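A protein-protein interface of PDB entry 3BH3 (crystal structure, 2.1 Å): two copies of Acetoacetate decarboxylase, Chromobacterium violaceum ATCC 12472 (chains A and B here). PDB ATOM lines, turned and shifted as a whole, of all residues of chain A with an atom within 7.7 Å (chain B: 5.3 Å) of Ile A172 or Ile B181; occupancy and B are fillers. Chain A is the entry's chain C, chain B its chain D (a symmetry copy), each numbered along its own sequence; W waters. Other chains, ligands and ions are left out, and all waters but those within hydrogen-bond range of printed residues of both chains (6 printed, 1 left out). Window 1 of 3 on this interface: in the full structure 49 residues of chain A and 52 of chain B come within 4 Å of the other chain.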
ATOM      1  N   ALA A  10      -2.552 -25.762  34.524  1.00  0.00           N
ATOM      2  CA  ALA A  10      -3.699 -25.623  33.626  1.00  0.00           C
ATOM      3  C   ALA A  10      -3.342 -25.096  32.222  1.00  0.00           C
ATOM      4  O   ALA A  10      -2.597 -24.127  32.062  1.00  0.00           O
ATOM      5  CB  ALA A  10      -4.795 -24.773  34.259  1.00  0.00           C
ATOM      6  N   PHE A  11      -3.860 -25.781  31.208  1.00  0.00           N
ATOM      7  CA  PHE A  11      -3.743 -25.341  29.820  1.00  0.00           C
ATOM      8  C   PHE A  11      -5.059 -25.638  29.085  1.00  0.00           C
ATOM      9  O   PHE A  11      -5.712 -24.730  28.609  1.00  0.00           O
ATOM     10  CB  PHE A  11      -2.519 -25.990  29.136  1.00  0.00           C
ATOM     11  CG  PHE A  11      -2.463 -25.770  27.653  1.00  0.00           C
ATOM     12  CD1 PHE A  11      -2.717 -26.826  26.767  1.00  0.00           C
ATOM     13  CD2 PHE A  11      -2.178 -24.511  27.132  1.00  0.00           C
ATOM     14  CE1 PHE A  11      -2.688 -26.631  25.376  1.00  0.00           C
ATOM     15  CE2 PHE A  11      -2.144 -24.298  25.734  1.00  0.00           C
ATOM     16  CZ  PHE A  11      -2.392 -25.370  24.857  1.00  0.00           C
ATOM     17  N   ALA A  12      -5.437 -26.916  29.016  1.00  0.00           N
ATOM     18  CA  ALA A  12      -6.673 -27.360  28.347  1.00  0.00           C
ATOM     19  C   ALA A  12      -7.259 -28.518  29.137  1.00  0.00           C
ATOM     20  O   ALA A  12      -6.534 -29.191  29.850  1.00  0.00           O
ATOM     21  CB  ALA A  12      -6.386 -27.808  26.929  1.00  0.00           C
ATOM     22  N   MET A  13      -8.559 -28.737  29.019  1.00  0.00           N
ATOM     23  CA  MET A  13      -9.204 -29.878  29.651  1.00  0.00           C
ATOM     24  C   MET A  13      -8.970 -31.167  28.852  1.00  0.00           C
ATOM     25  O   MET A  13      -8.838 -31.106  27.624  1.00  0.00           O
ATOM     26  CB  MET A  13     -10.698 -29.628  29.728  1.00  0.00           C
ATOM     27  CG  MET A  13     -11.072 -28.349  30.453  1.00  0.00           C
ATOM     28  SD  MET A  13     -12.829 -28.083  30.400  1.00  0.00           S
ATOM     29  CE  MET A  13     -13.011 -27.224  28.827  1.00  0.00           C
ATOM     30  N   ALA A 106     -10.923 -28.840  18.868  1.00  0.00           N
ATOM     31  CA  ALA A 106     -11.008 -28.265  20.202  1.00  0.00           C
ATOM     32  C   ALA A 106      -9.948 -27.177  20.356  1.00  0.00           C
ATOM     33  O   ALA A 106     -10.235 -26.081  20.817  1.00  0.00           O
ATOM     34  CB  ALA A 106     -10.851 -29.351  21.283  1.00  0.00           C
ATOM     35  N   ARG A 109     -10.901 -23.986  18.301  1.00  0.00           N
ATOM     36  CA  ARG A 109     -11.969 -23.242  18.995  1.00  0.00           C
ATOM     37  C   ARG A 109     -11.487 -22.557  20.283  1.00  0.00           C
ATOM     38  O   ARG A 109     -11.710 -21.372  20.503  1.00  0.00           O
ATOM     39  CB  ARG A 109     -13.134 -24.177  19.310  1.00  0.00           C
ATOM     40  CG  ARG A 109     -13.946 -24.558  18.073  1.00  0.00           C
ATOM     41  CD  ARG A 109     -15.115 -25.431  18.404  1.00  0.00           C
ATOM     42  NE  ARG A 109     -16.183 -24.689  19.076  1.00  0.00           N
ATOM     43  CZ  ARG A 109     -17.108 -23.951  18.478  1.00  0.00           C
ATOM     44  NH1 ARG A 109     -17.136 -23.823  17.163  1.00  0.00           N
ATOM     45  NH2 ARG A 109     -18.020 -23.322  19.211  1.00  0.00           N
ATOM     46  N   GLU A 110     -10.792 -23.312  21.117  1.00  0.00           N
ATOM     47  CA  GLU A 110     -10.569 -22.892  22.487  1.00  0.00           C
ATOM     48  C   GLU A 110      -9.403 -21.941  22.614  1.00  0.00           C
ATOM     49  O   GLU A 110      -9.398 -21.076  23.509  1.00  0.00           O
ATOM     50  CB  GLU A 110     -10.416 -24.102  23.398  1.00  0.00           C
ATOM     51  CG  GLU A 110     -11.770 -24.759  23.690  1.00  0.00           C
ATOM     52  CD  GLU A 110     -11.662 -26.200  24.190  1.00  0.00           C
ATOM     53  OE1 GLU A 110     -10.657 -26.556  24.868  1.00  0.00           O
ATOM     54  OE2 GLU A 110     -12.601 -26.980  23.909  1.00  0.00           O
ATOM     55  N   LEU A 111      -8.446 -22.071  21.696  1.00  0.00           N
ATOM     56  CA  LEU A 111      -7.231 -21.288  21.757  1.00  0.00           C
ATOM     57  C   LEU A 111      -7.234 -20.019  20.883  1.00  0.00           C
ATOM     58  O   LEU A 111      -7.026 -18.932  21.428  1.00  0.00           O
ATOM     59  CB  LEU A 111      -6.010 -22.177  21.545  1.00  0.00           C
ATOM     60  CG  LEU A 111      -4.597 -21.642  21.691  1.00  0.00           C
ATOM     61  CD1 LEU A 111      -4.327 -21.074  23.060  1.00  0.00           C
ATOM     62  CD2 LEU A 111      -3.664 -22.793  21.444  1.00  0.00           C
ATOM     63  N   GLY A 113      -9.895 -19.376  18.669  1.00  0.00           N
ATOM     64  CA  GLY A 113     -11.269 -19.033  18.344  1.00  0.00           C
ATOM     65  C   GLY A 113     -11.609 -19.222  16.872  1.00  0.00           C
ATOM     66  O   GLY A 113     -12.365 -18.428  16.282  1.00  0.00           O
ATOM     67  N   LEU A 169     -13.541 -14.128  15.329  1.00  0.00           N
ATOM     68  CA  LEU A 169     -14.363 -13.782  16.487  1.00  0.00           C
ATOM     69  C   LEU A 169     -14.453 -14.927  17.500  1.00  0.00           C
ATOM     70  O   LEU A 169     -15.338 -15.790  17.407  1.00  0.00           O
ATOM     71  CB  LEU A 169     -15.763 -13.268  16.086  1.00  0.00           C
ATOM     72  CG  LEU A 169     -16.781 -12.905  17.197  1.00  0.00           C
ATOM     73  CD1 LEU A 169     -16.268 -11.871  18.239  1.00  0.00           C
ATOM     74  CD2 LEU A 169     -18.162 -12.443  16.624  1.00  0.00           C
ATOM     75  N   LYS A 170     -13.534 -14.908  18.471  1.00  0.00           N
ATOM     76  CA  LYS A 170     -13.575 -15.838  19.604  1.00  0.00           C
ATOM     77  C   LYS A 170     -14.721 -15.532  20.593  1.00  0.00           C
ATOM     78  O   LYS A 170     -14.752 -14.465  21.215  1.00  0.00           O
ATOM     79  CB  LYS A 170     -12.220 -15.876  20.333  1.00  0.00           C
ATOM     80  CG  LYS A 170     -12.124 -16.957  21.401  1.00  0.00           C
ATOM     81  CD  LYS A 170     -10.788 -16.912  22.094  1.00  0.00           C
ATOM     82  CE  LYS A 170     -10.575 -18.159  22.923  1.00  0.00           C
ATOM     83  NZ  LYS A 170      -9.214 -18.185  23.547  1.00  0.00           N
ATOM     84  N   ILE A 171     -15.653 -16.479  20.714  1.00  0.00           N
ATOM     85  CA  ILE A 171     -16.735 -16.456  21.697  1.00  0.00           C
ATOM     86  C   ILE A 171     -16.666 -17.736  22.536  1.00  0.00           C
ATOM     87  O   ILE A 171     -16.534 -18.835  21.984  1.00  0.00           O
ATOM     88  CB  ILE A 171     -18.128 -16.406  21.039  1.00  0.00           C
ATOM     89  CG1 ILE A 171     -18.195 -15.337  19.925  1.00  0.00           C
ATOM     90  CG2 ILE A 171     -19.199 -16.160  22.080  1.00  0.00           C
ATOM     91  CD1 ILE A 171     -19.554 -15.318  19.161  1.00  0.00           C
ATOM     92  N   ILE A 172     -16.732 -17.579  23.860  1.00  0.00           N
ATOM     93  CA  ILE A 172     -16.847 -18.698  24.804  1.00  0.00           C
ATOM     94  C   ILE A 172     -17.886 -18.311  25.857  1.00  0.00           C
ATOM     95  O   ILE A 172     -17.756 -17.261  26.496  1.00  0.00           O
ATOM     96  CB  ILE A 172     -15.481 -19.096  25.470  1.00  0.00           C
ATOM     97  CG1 ILE A 172     -14.409 -19.428  24.419  1.00  0.00           C
ATOM     98  CG2 ILE A 172     -15.663 -20.247  26.464  1.00  0.00           C
ATOM     99  CD1 ILE A 172     -14.583 -20.807  23.678  1.00  0.00           C
ATOM    100  N   PRO A 173     -18.955 -19.114  25.988  1.00  0.00           N
ATOM    101  CA  PRO A 173     -19.969 -18.877  27.017  1.00  0.00           C
ATOM    102  C   PRO A 173     -19.441 -19.106  28.423  1.00  0.00           C
ATOM    103  O   PRO A 173     -18.483 -19.861  28.623  1.00  0.00           O
ATOM    104  CB  PRO A 173     -21.046 -19.920  26.700  1.00  0.00           C
ATOM    105  CG  PRO A 173     -20.310 -21.004  25.961  1.00  0.00           C
ATOM    106  CD  PRO A 173     -19.302 -20.264  25.135  1.00  0.00           C
ATOM    107  N   HIS A 174     -20.061 -18.425  29.382  1.00  0.00           N
ATOM    108  CA  HIS A 174     -19.782 -18.645  30.798  1.00  0.00           C
ATOM    109  C   HIS A 174     -20.721 -19.773  31.179  1.00  0.00           C
ATOM    110  O   HIS A 174     -21.671 -20.058  30.433  1.00  0.00           O
ATOM    111  CB  HIS A 174     -20.055 -17.364  31.614  1.00  0.00           C
ATOM    112  CG  HIS A 174     -19.689 -17.466  33.066  1.00  0.00           C
ATOM    113  ND1 HIS A 174     -18.432 -17.837  33.499  1.00  0.00           N
ATOM    114  CD2 HIS A 174     -20.416 -17.227  34.184  1.00  0.00           C
ATOM    115  CE1 HIS A 174     -18.404 -17.836  34.820  1.00  0.00           C
ATOM    116  NE2 HIS A 174     -19.593 -17.468  35.259  1.00  0.00           N
ATOM    117  N   VAL A 175     -20.455 -20.425  32.317  1.00  0.00           N
ATOM    118  CA  VAL A 175     -21.290 -21.549  32.766  1.00  0.00           C
ATOM    119  C   VAL A 175     -22.804 -21.252  32.688  1.00  0.00           C
ATOM    120  O   VAL A 175     -23.614 -22.168  32.581  1.00  0.00           O
ATOM    121  CB  VAL A 175     -20.857 -22.068  34.157  1.00  0.00           C
ATOM    122  CG1 VAL A 175     -19.416 -22.501  34.113  1.00  0.00           C
ATOM    123  CG2 VAL A 175     -21.048 -20.987  35.254  1.00  0.00           C
ATOM    124  N   GLY A 177     -24.299 -19.322  30.276  1.00  0.00           N
ATOM    125  CA  GLY A 177     -24.733 -19.121  28.903  1.00  0.00           C
ATOM    126  C   GLY A 177     -24.425 -17.757  28.330  1.00  0.00           C
ATOM    127  O   GLY A 177     -24.522 -17.554  27.135  1.00  0.00           O
ATOM    128  N   SER A 178     -24.054 -16.810  29.181  1.00  0.00           N
ATOM    129  CA  SER A 178     -23.704 -15.470  28.711  1.00  0.00           C
ATOM    130  C   SER A 178     -22.217 -15.420  28.372  1.00  0.00           C
ATOM    131  O   SER A 178     -21.418 -16.116  29.010  1.00  0.00           O
ATOM    132  CB  SER A 178     -24.060 -14.424  29.773  1.00  0.00           C
ATOM    133  OG  SER A 178     -23.220 -14.533  30.915  1.00  0.00           O
ATOM    134  N   PRO A 179     -21.833 -14.611  27.365  1.00  0.00           N
ATOM    135  CA  PRO A 179     -20.431 -14.545  26.930  1.00  0.00           C
ATOM    136  C   PRO A 179     -19.438 -14.251  28.041  1.00  0.00           C
ATOM    137  O   PRO A 179     -19.579 -13.256  28.761  1.00  0.00           O
ATOM    138  CB  PRO A 179     -20.424 -13.400  25.915  1.00  0.00           C
ATOM    139  CG  PRO A 179     -21.808 -13.347  25.409  1.00  0.00           C
ATOM    140  CD  PRO A 179     -22.699 -13.741  26.547  1.00  0.00           C
ATOM    141  N   ARG A 180     -18.450 -15.129  28.154  1.00  0.00           N
ATOM    142  CA  ARG A 180     -17.322 -14.974  29.049  1.00  0.00           C
ATOM    143  C   ARG A 180     -16.094 -14.467  28.260  1.00  0.00           C
ATOM    144  O   ARG A 180     -15.375 -13.567  28.703  1.00  0.00           O
ATOM    145  CB  ARG A 180     -17.044 -16.310  29.758  1.00  0.00           C
ATOM    146  CG  ARG A 180     -15.820 -16.348  30.657  1.00  0.00           C
ATOM    147  CD  ARG A 180     -15.980 -15.578  31.980  1.00  0.00           C
ATOM    148  NE  ARG A 180     -14.733 -15.642  32.746  1.00  0.00           N
ATOM    149  CZ  ARG A 180     -14.419 -16.616  33.601  1.00  0.00           C
ATOM    150  NH1 ARG A 180     -15.261 -17.630  33.837  1.00  0.00           N
ATOM    151  NH2 ARG A 180     -13.261 -16.581  34.230  1.00  0.00           N
ATOM    152  N   ILE A 181     -15.863 -15.049  27.088  1.00  0.00           N
ATOM    153  CA  ILE A 181     -14.916 -14.512  26.126  1.00  0.00           C
ATOM    154  C   ILE A 181     -15.729 -14.029  24.920  1.00  0.00           C
ATOM    155  O   ILE A 181     -16.731 -14.635  24.538  1.00  0.00           O
ATOM    156  CB  ILE A 181     -13.860 -15.553  25.740  1.00  0.00           C
ATOM    157  CG1 ILE A 181     -13.071 -15.967  26.991  1.00  0.00           C
ATOM    158  CG2 ILE A 181     -12.935 -15.024  24.659  1.00  0.00           C
ATOM    159  CD1 ILE A 181     -12.169 -17.194  26.834  1.00  0.00           C
ATOM    160  N   CYS A 182     -15.344 -12.885  24.369  1.00  0.00           N
ATOM    161  CA  CYS A 182     -15.980 -12.385  23.161  1.00  0.00           C
ATOM    162  C   CYS A 182     -15.124 -11.268  22.601  1.00  0.00           C
ATOM    163  O   CYS A 182     -15.323 -10.088  22.896  1.00  0.00           O
ATOM    164  CB  CYS A 182     -17.413 -11.952  23.418  1.00  0.00           C
ATOM    165  SG  CYS A 182     -18.294 -11.494  21.914  1.00  0.00           S
ATOM    166  N   GLU A 183     -14.132 -11.674  21.817  1.00  0.00           N
ATOM    167  CA  GLU A 183     -13.138 -10.762  21.271  1.00  0.00           C
ATOM    168  C   GLU A 183     -12.858 -11.009  19.799  1.00  0.00           C
ATOM    169  O   GLU A 183     -13.091 -12.107  19.294  1.00  0.00           O
ATOM    170  CB  GLU A 183     -11.838 -10.925  22.050  1.00  0.00           C
ATOM    171  CG  GLU A 183     -11.512 -12.362  22.373  1.00  0.00           C
ATOM    172  CD  GLU A 183     -10.797 -12.522  23.703  1.00  0.00           C
ATOM    173  OE1 GLU A 183     -11.183 -11.830  24.683  1.00  0.00           O
ATOM    174  OE2 GLU A 183      -9.863 -13.358  23.770  1.00  0.00           O
ATOM    175  N   LEU A 244     -16.108  -6.988  25.501  1.00  0.00           N
ATOM    176  CA  LEU A 244     -16.562  -6.949  26.883  1.00  0.00           C
ATOM    177  C   LEU A 244     -15.863  -5.866  27.727  1.00  0.00           C
ATOM    178  O   LEU A 244     -15.021  -5.094  27.228  1.00  0.00           O
ATOM    179  CB  LEU A 244     -16.401  -8.341  27.516  1.00  0.00           C
ATOM    180  CG  LEU A 244     -17.384  -9.511  27.250  1.00  0.00           C
ATOM    181  CD1 LEU A 244     -18.360  -9.347  26.078  1.00  0.00           C
ATOM    182  CD2 LEU A 244     -16.598 -10.823  27.119  1.00  0.00           C
ATOM    183  N   PHE B  11     -23.236 -16.283  21.775  1.00  0.00           N
ATOM    184  CA  PHE B  11     -23.415 -17.424  22.674  1.00  0.00           C
ATOM    185  C   PHE B  11     -22.266 -18.444  22.433  1.00  0.00           C
ATOM    186  O   PHE B  11     -21.406 -18.646  23.306  1.00  0.00           O
ATOM    187  CB  PHE B  11     -24.829 -18.024  22.533  1.00  0.00           C
ATOM    188  CG  PHE B  11     -24.998 -19.344  23.218  1.00  0.00           C
ATOM    189  CD1 PHE B  11     -25.062 -20.531  22.471  1.00  0.00           C
ATOM    190  CD2 PHE B  11     -25.074 -19.421  24.613  1.00  0.00           C
ATOM    191  CE1 PHE B  11     -25.188 -21.759  23.108  1.00  0.00           C
ATOM    192  CE2 PHE B  11     -25.197 -20.641  25.256  1.00  0.00           C
ATOM    193  CZ  PHE B  11     -25.251 -21.813  24.515  1.00  0.00           C
ATOM    194  N   MET B  13     -19.374 -19.858  19.106  1.00  0.00           N
ATOM    195  CA  MET B  13     -18.863 -19.744  17.729  1.00  0.00           C
ATOM    196  C   MET B  13     -19.392 -20.860  16.830  1.00  0.00           C
ATOM    197  O   MET B  13     -19.675 -21.960  17.304  1.00  0.00           O
ATOM    198  CB  MET B  13     -17.346 -19.811  17.696  1.00  0.00           C
ATOM    199  CG  MET B  13     -16.636 -18.973  18.716  1.00  0.00           C
ATOM    200  SD  MET B  13     -14.884 -19.324  18.635  1.00  0.00           S
ATOM    201  CE  MET B  13     -14.727 -20.698  19.781  1.00  0.00           C
ATOM    202  N   GLU B 110     -17.163 -26.129  26.305  1.00  0.00           N
ATOM    203  CA  GLU B 110     -17.168 -24.684  26.298  1.00  0.00           C
ATOM    204  C   GLU B 110     -18.094 -24.086  27.377  1.00  0.00           C
ATOM    205  O   GLU B 110     -17.808 -23.013  27.934  1.00  0.00           O
ATOM    206  CB  GLU B 110     -17.499 -24.190  24.898  1.00  0.00           C
ATOM    207  CG  GLU B 110     -16.258 -24.212  24.015  1.00  0.00           C
ATOM    208  CD  GLU B 110     -16.538 -24.271  22.520  1.00  0.00           C
ATOM    209  OE1 GLU B 110     -17.426 -23.550  22.035  1.00  0.00           O
ATOM    210  OE2 GLU B 110     -15.818 -25.015  21.821  1.00  0.00           O
ATOM    211  N   LYS B 170     -13.397 -26.607  34.904  1.00  0.00           N
ATOM    212  CA  LYS B 170     -13.444 -25.880  33.630  1.00  0.00           C
ATOM    213  C   LYS B 170     -12.171 -25.072  33.374  1.00  0.00           C
ATOM    214  O   LYS B 170     -11.822 -24.167  34.158  1.00  0.00           O
ATOM    215  CB  LYS B 170     -14.662 -24.970  33.547  1.00  0.00           C
ATOM    216  CG  LYS B 170     -14.815 -24.305  32.191  1.00  0.00           C
ATOM    217  CD  LYS B 170     -16.162 -23.630  32.071  1.00  0.00           C
ATOM    218  CE  LYS B 170     -16.271 -22.820  30.770  1.00  0.00           C
ATOM    219  NZ  LYS B 170     -17.623 -22.205  30.626  1.00  0.00           N
ATOM    220  N   ILE B 171     -11.486 -25.414  32.279  1.00  0.00           N
ATOM    221  CA  ILE B 171     -10.265 -24.725  31.836  1.00  0.00           C
ATOM    222  C   ILE B 171     -10.370 -24.353  30.357  1.00  0.00           C
ATOM    223  O   ILE B 171     -10.609 -25.232  29.521  1.00  0.00           O
ATOM    224  CB  ILE B 171      -9.014 -25.612  31.955  1.00  0.00           C
ATOM    225  CG1 ILE B 171      -8.957 -26.347  33.290  1.00  0.00           C
ATOM    226  CG2 ILE B 171      -7.750 -24.785  31.689  1.00  0.00           C
ATOM    227  CD1 ILE B 171      -7.903 -27.463  33.300  1.00  0.00           C
ATOM    228  N   ILE B 172     -10.196 -23.069  30.044  1.00  0.00           N
ATOM    229  CA  ILE B 172     -10.121 -22.584  28.663  1.00  0.00           C
ATOM    230  C   ILE B 172      -8.885 -21.695  28.517  1.00  0.00           C
ATOM    231  O   ILE B 172      -8.710 -20.763  29.292  1.00  0.00           O
ATOM    232  CB  ILE B 172     -11.368 -21.760  28.253  1.00  0.00           C
ATOM    233  CG1 ILE B 172     -12.650 -22.611  28.282  1.00  0.00           C
ATOM    234  CG2 ILE B 172     -11.146 -21.064  26.878  1.00  0.00           C
ATOM    235  CD1 ILE B 172     -12.791 -23.656  27.161  1.00  0.00           C
ATOM    236  N   PRO B 179      -4.106 -19.745  31.147  1.00  0.00           N
ATOM    237  CA  PRO B 179      -5.548 -19.924  31.368  1.00  0.00           C
ATOM    238  C   PRO B 179      -6.387 -18.643  31.502  1.00  0.00           C
ATOM    239  O   PRO B 179      -6.036 -17.736  32.240  1.00  0.00           O
ATOM    240  CB  PRO B 179      -5.620 -20.806  32.621  1.00  0.00           C
ATOM    241  CG  PRO B 179      -4.283 -20.690  33.272  1.00  0.00           C
ATOM    242  CD  PRO B 179      -3.287 -20.301  32.242  1.00  0.00           C
ATOM    243  N   ARG B 180      -7.492 -18.595  30.764  1.00  0.00           N
ATOM    244  CA  ARG B 180      -8.415 -17.477  30.785  1.00  0.00           C
ATOM    245  C   ARG B 180      -9.624 -17.860  31.632  1.00  0.00           C
ATOM    246  O   ARG B 180     -10.198 -17.021  32.335  1.00  0.00           O
ATOM    247  CB  ARG B 180      -8.840 -17.122  29.347  1.00  0.00           C
ATOM    248  CG  ARG B 180      -9.890 -16.038  29.206  1.00  0.00           C
ATOM    249  CD  ARG B 180      -9.315 -14.614  29.238  1.00  0.00           C
ATOM    250  NE  ARG B 180     -10.430 -13.677  29.131  1.00  0.00           N
ATOM    251  CZ  ARG B 180     -10.822 -13.058  28.014  1.00  0.00           C
ATOM    252  NH1 ARG B 180     -10.182 -13.244  26.852  1.00  0.00           N
ATOM    253  NH2 ARG B 180     -11.876 -12.251  28.064  1.00  0.00           N
ATOM    254  N   ILE B 181     -10.023 -19.122  31.541  1.00  0.00           N
ATOM    255  CA  ILE B 181     -11.033 -19.661  32.434  1.00  0.00           C
ATOM    256  C   ILE B 181     -10.358 -20.791  33.185  1.00  0.00           C
ATOM    257  O   ILE B 181      -9.685 -21.620  32.575  1.00  0.00           O
ATOM    258  CB  ILE B 181     -12.280 -20.176  31.696  1.00  0.00           C
ATOM    259  CG1 ILE B 181     -12.914 -19.055  30.869  1.00  0.00           C
ATOM    260  CG2 ILE B 181     -13.292 -20.761  32.704  1.00  0.00           C
ATOM    261  CD1 ILE B 181     -14.085 -19.496  29.981  1.00  0.00           C
ATOM    262  N   CYS B 182     -10.478 -20.784  34.512  1.00  0.00           N
ATOM    263  CA  CYS B 182      -9.964 -21.884  35.330  1.00  0.00           C
ATOM    264  C   CYS B 182     -10.698 -21.894  36.649  1.00  0.00           C
ATOM    265  O   CYS B 182     -10.302 -21.203  37.601  1.00  0.00           O
ATOM    266  CB  CYS B 182      -8.467 -21.783  35.547  1.00  0.00           C
ATOM    267  SG  CYS B 182      -7.792 -23.274  36.248  1.00  0.00           S
ATOM    268  N   GLU B 183     -11.780 -22.669  36.681  1.00  0.00           N
ATOM    269  CA  GLU B 183     -12.706 -22.699  37.804  1.00  0.00           C
ATOM    270  C   GLU B 183     -13.288 -24.094  38.028  1.00  0.00           C
ATOM    271  O   GLU B 183     -13.326 -24.900  37.097  1.00  0.00           O
ATOM    272  CB  GLU B 183     -13.836 -21.691  37.564  1.00  0.00           C
ATOM    273  CG  GLU B 183     -14.604 -21.873  36.257  1.00  0.00           C
ATOM    274  CD  GLU B 183     -15.116 -20.565  35.669  1.00  0.00           C
ATOM    275  OE1 GLU B 183     -14.399 -19.519  35.733  1.00  0.00           O
ATOM    276  OE2 GLU B 183     -16.241 -20.593  35.132  1.00  0.00           O
ATOM    277  N   LEU B 244      -8.684 -18.251  39.402  1.00  0.00           N
ATOM    278  CA  LEU B 244      -8.058 -17.017  38.884  1.00  0.00           C
ATOM    279  C   LEU B 244      -8.668 -15.723  39.479  1.00  0.00           C
ATOM    280  O   LEU B 244      -8.578 -14.647  38.863  1.00  0.00           O
ATOM    281  CB  LEU B 244      -8.137 -16.968  37.341  1.00  0.00           C
ATOM    282  CG  LEU B 244      -7.661 -18.152  36.480  1.00  0.00           C
ATOM    283  CD1 LEU B 244      -8.049 -17.915  35.030  1.00  0.00           C
ATOM    284  CD2 LEU B 244      -6.148 -18.427  36.621  1.00  0.00           C
HETATM  285  O   HOH W   1      -9.644 -26.376  27.292  1.00  0.00           O
HETATM  286  O   HOH W   2      -9.199 -15.662  24.739  1.00  0.00           O
HETATM  287  O   HOH W   3     -13.590 -11.020  25.442  1.00  0.00           O
HETATM  288  O   HOH W   4     -16.909 -19.887  32.662  1.00  0.00           O
HETATM  289  O   HOH W   5     -18.082 -20.950  21.848  1.00  0.00           O
HETATM  290  O   HOH W   6     -14.448 -27.119  21.864  1.00  0.00           O
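A ring nitrogen (ND1) of His A174 lies within hydrogen-bond range of the guanidinium group of Arg A180, 3.2 Å away.
The backbone carbonyl oxygen (O) of Ile B181 sits at hydrogen-bond distance from the backbone NH (N) of Ile B172, at 3.0 Å.
NZ of Lys B170 sits at hydrogen-bond distance from O of Glu B110 (2.8 Å).
N of Ile A181 sits at hydrogen-bond distance from O of Ile A172 (3.0 Å).
O of Ala A10 touches CD of Pro B179, 3.9 Å away.
CG of Glu A110 touches CD1 of Ile B172, at 3.8 Å.
Ile A172 touches Glu B110 (CG2 to O, 3.8 Å).
Ile A172 touches Ile B181 (CG2 to CD1, 3.9 Å).
O of Phe B11 touches CD of Pro A173, 3.2 Å away.
His A174 touches Lys B170.
Glu B183 touches Val A175 (OE2 to CG1, 3.8 Å).
O of Arg B180 touches NH2 of Arg A180, at 3.6 Å.
Arg A180 touches Ile B181 (CG to CD1, 3.7 Å).
Ile A181 touches Arg B180 (CD1 to CG, 3.5 Å).
Printed residues of chain A that touch a printed residue of chain B: Ala A10, Phe A11, Met A13, Arg A109, Glu A110, Gly A113, Leu A169, Lys A170, Ile A171, Ile A172, Pro A173, His A174, Val A175, Gly A177, Arg A180, Ile A181 and Glu A183.
Hydrophobic or aromatic side chains of chain A within 4 Å of the printed part of chain B: Ala A10, Met A13, Ile A171, Ile A172, Pro A173, His A174, Val A175 and Ile A181.
Printed residues of chain B that touch a printed residue of chain A: Phe B11, Met B13, Glu B110, Lys B170, Ile B171, Ile B172, Pro B179, Arg B180, Ile B181, Cys B182 and Glu B183.
Hydrophobic or aromatic side chains of chain B within 4 Å of the printed part of chain A: Phe B11, Met B13, Ile B171, Ile B172, Pro B179 and Ile B181.
Among the printed residues, 31 pairs touch across the chains.
Among the printed residues, Asp or Glu carboxylates within 4 Å of a Lys or Arg side-chain nitrogen of the other chain: Arg A109 with Glu B110, Arg A180 with Glu B183 and Glu A183 with Arg B180.
Water W6 bridges the side-chain carboxylate of Glu B110 (2.5 Å) and the side-chain carboxylate of Glu A110 (2.8 Å).
Water W2 lies within hydrogen-bond range of the side-chain carboxylate (OE2) of Glu A183 (2.6 Å), the side-chain amino group (NZ) of Lys A170 (2.8 Å) and the guanidinium group (NH1) of Arg B180 (3.4 Å).
Water W5 lies within hydrogen-bond range of O of Ile A171 (2.6 Å), OE1 of Glu B110 (2.7 Å) and N of Met B13 (3.2 Å).
Phe A11 touches Ile B171, and with the chains exchanged Ile A171 touches Phe B11.
Met A13 touches Lys B170, and with the chains exchanged Lys A170 touches Met B13.
Met A13 touches Ile B171, and with the chains exchanged Ile A171 touches Met B13.
Arg A180 touches Ile B181, and with the chains exchanged Ile A181 touches Arg B180.
12 positions are printed for both chains.
Of the 31 pairs that touch across the chains among the printed residues, 15 have their exchanged pair printed and touching as well.
The side-chain carboxylate (OE2) of Glu B110 is in salt-bridge range of the guanidinium group (NE) of Arg A109.
The guanidinium group (NH1) of Arg A180 lies within salt-bridge range of the side-chain carboxylate (OE1) of Glu B183 (2.8 Å).
O of Pro A173 lies within hydrogen-bond range of NZ of Lys B170, at 3.2 Å.
The backbone NH of Ile A171 sits close to the side-chain sulfur of Met B13, 3.6 Å away.
The backbone carbonyl oxygen of Gly A113 sits close to the side-chain sulfur of Met B13 (3.6 Å).
NH1 of Arg B180 lies within salt-bridge range of OE1 of Glu A183 (2.8 Å).
The side-chain sulfur of Met A13 lies close to the backbone NH of Ile B171, 3.5 Å away.
The backbone carbonyl oxygen (O) of Glu B110 lies close to the backbone carbonyl oxygen (O) of Pro A173 (3.3 Å).
The backbone carbonyl oxygen (O) of Leu A169 lies close to the side-chain sulfur (SD) of Met B13.
The guanidinium group of Arg A109 lies within hydrogen-bond range of the backbone carbonyl oxygen of Met B13.
Of chain B, only Met B13, Glu B110 and Ile B181 come within 4 Å of Ile A172.
Of the printed residues of chain A, Ile B181 touches Ile A172 and Arg A180.
Of the printed residues of chain B, Ile A171 touches Phe B11 and Met B13.
Printed residues of chain B within 4 Å of Gly A113: Met B13.
Of the printed residues of chain A, Pro B179 touches Ala A10 (3.9 Å).
The nearest residue of chain B that does not touch Ile A172 is Ile B172 (4.2 Å).
The nearest residue of chain A that does not touch Ile B181 is Ile A181 (4.3 Å).
The nearest printed residue of chain B that does not touch Gly A113 is Glu B110 (8.3 Å).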
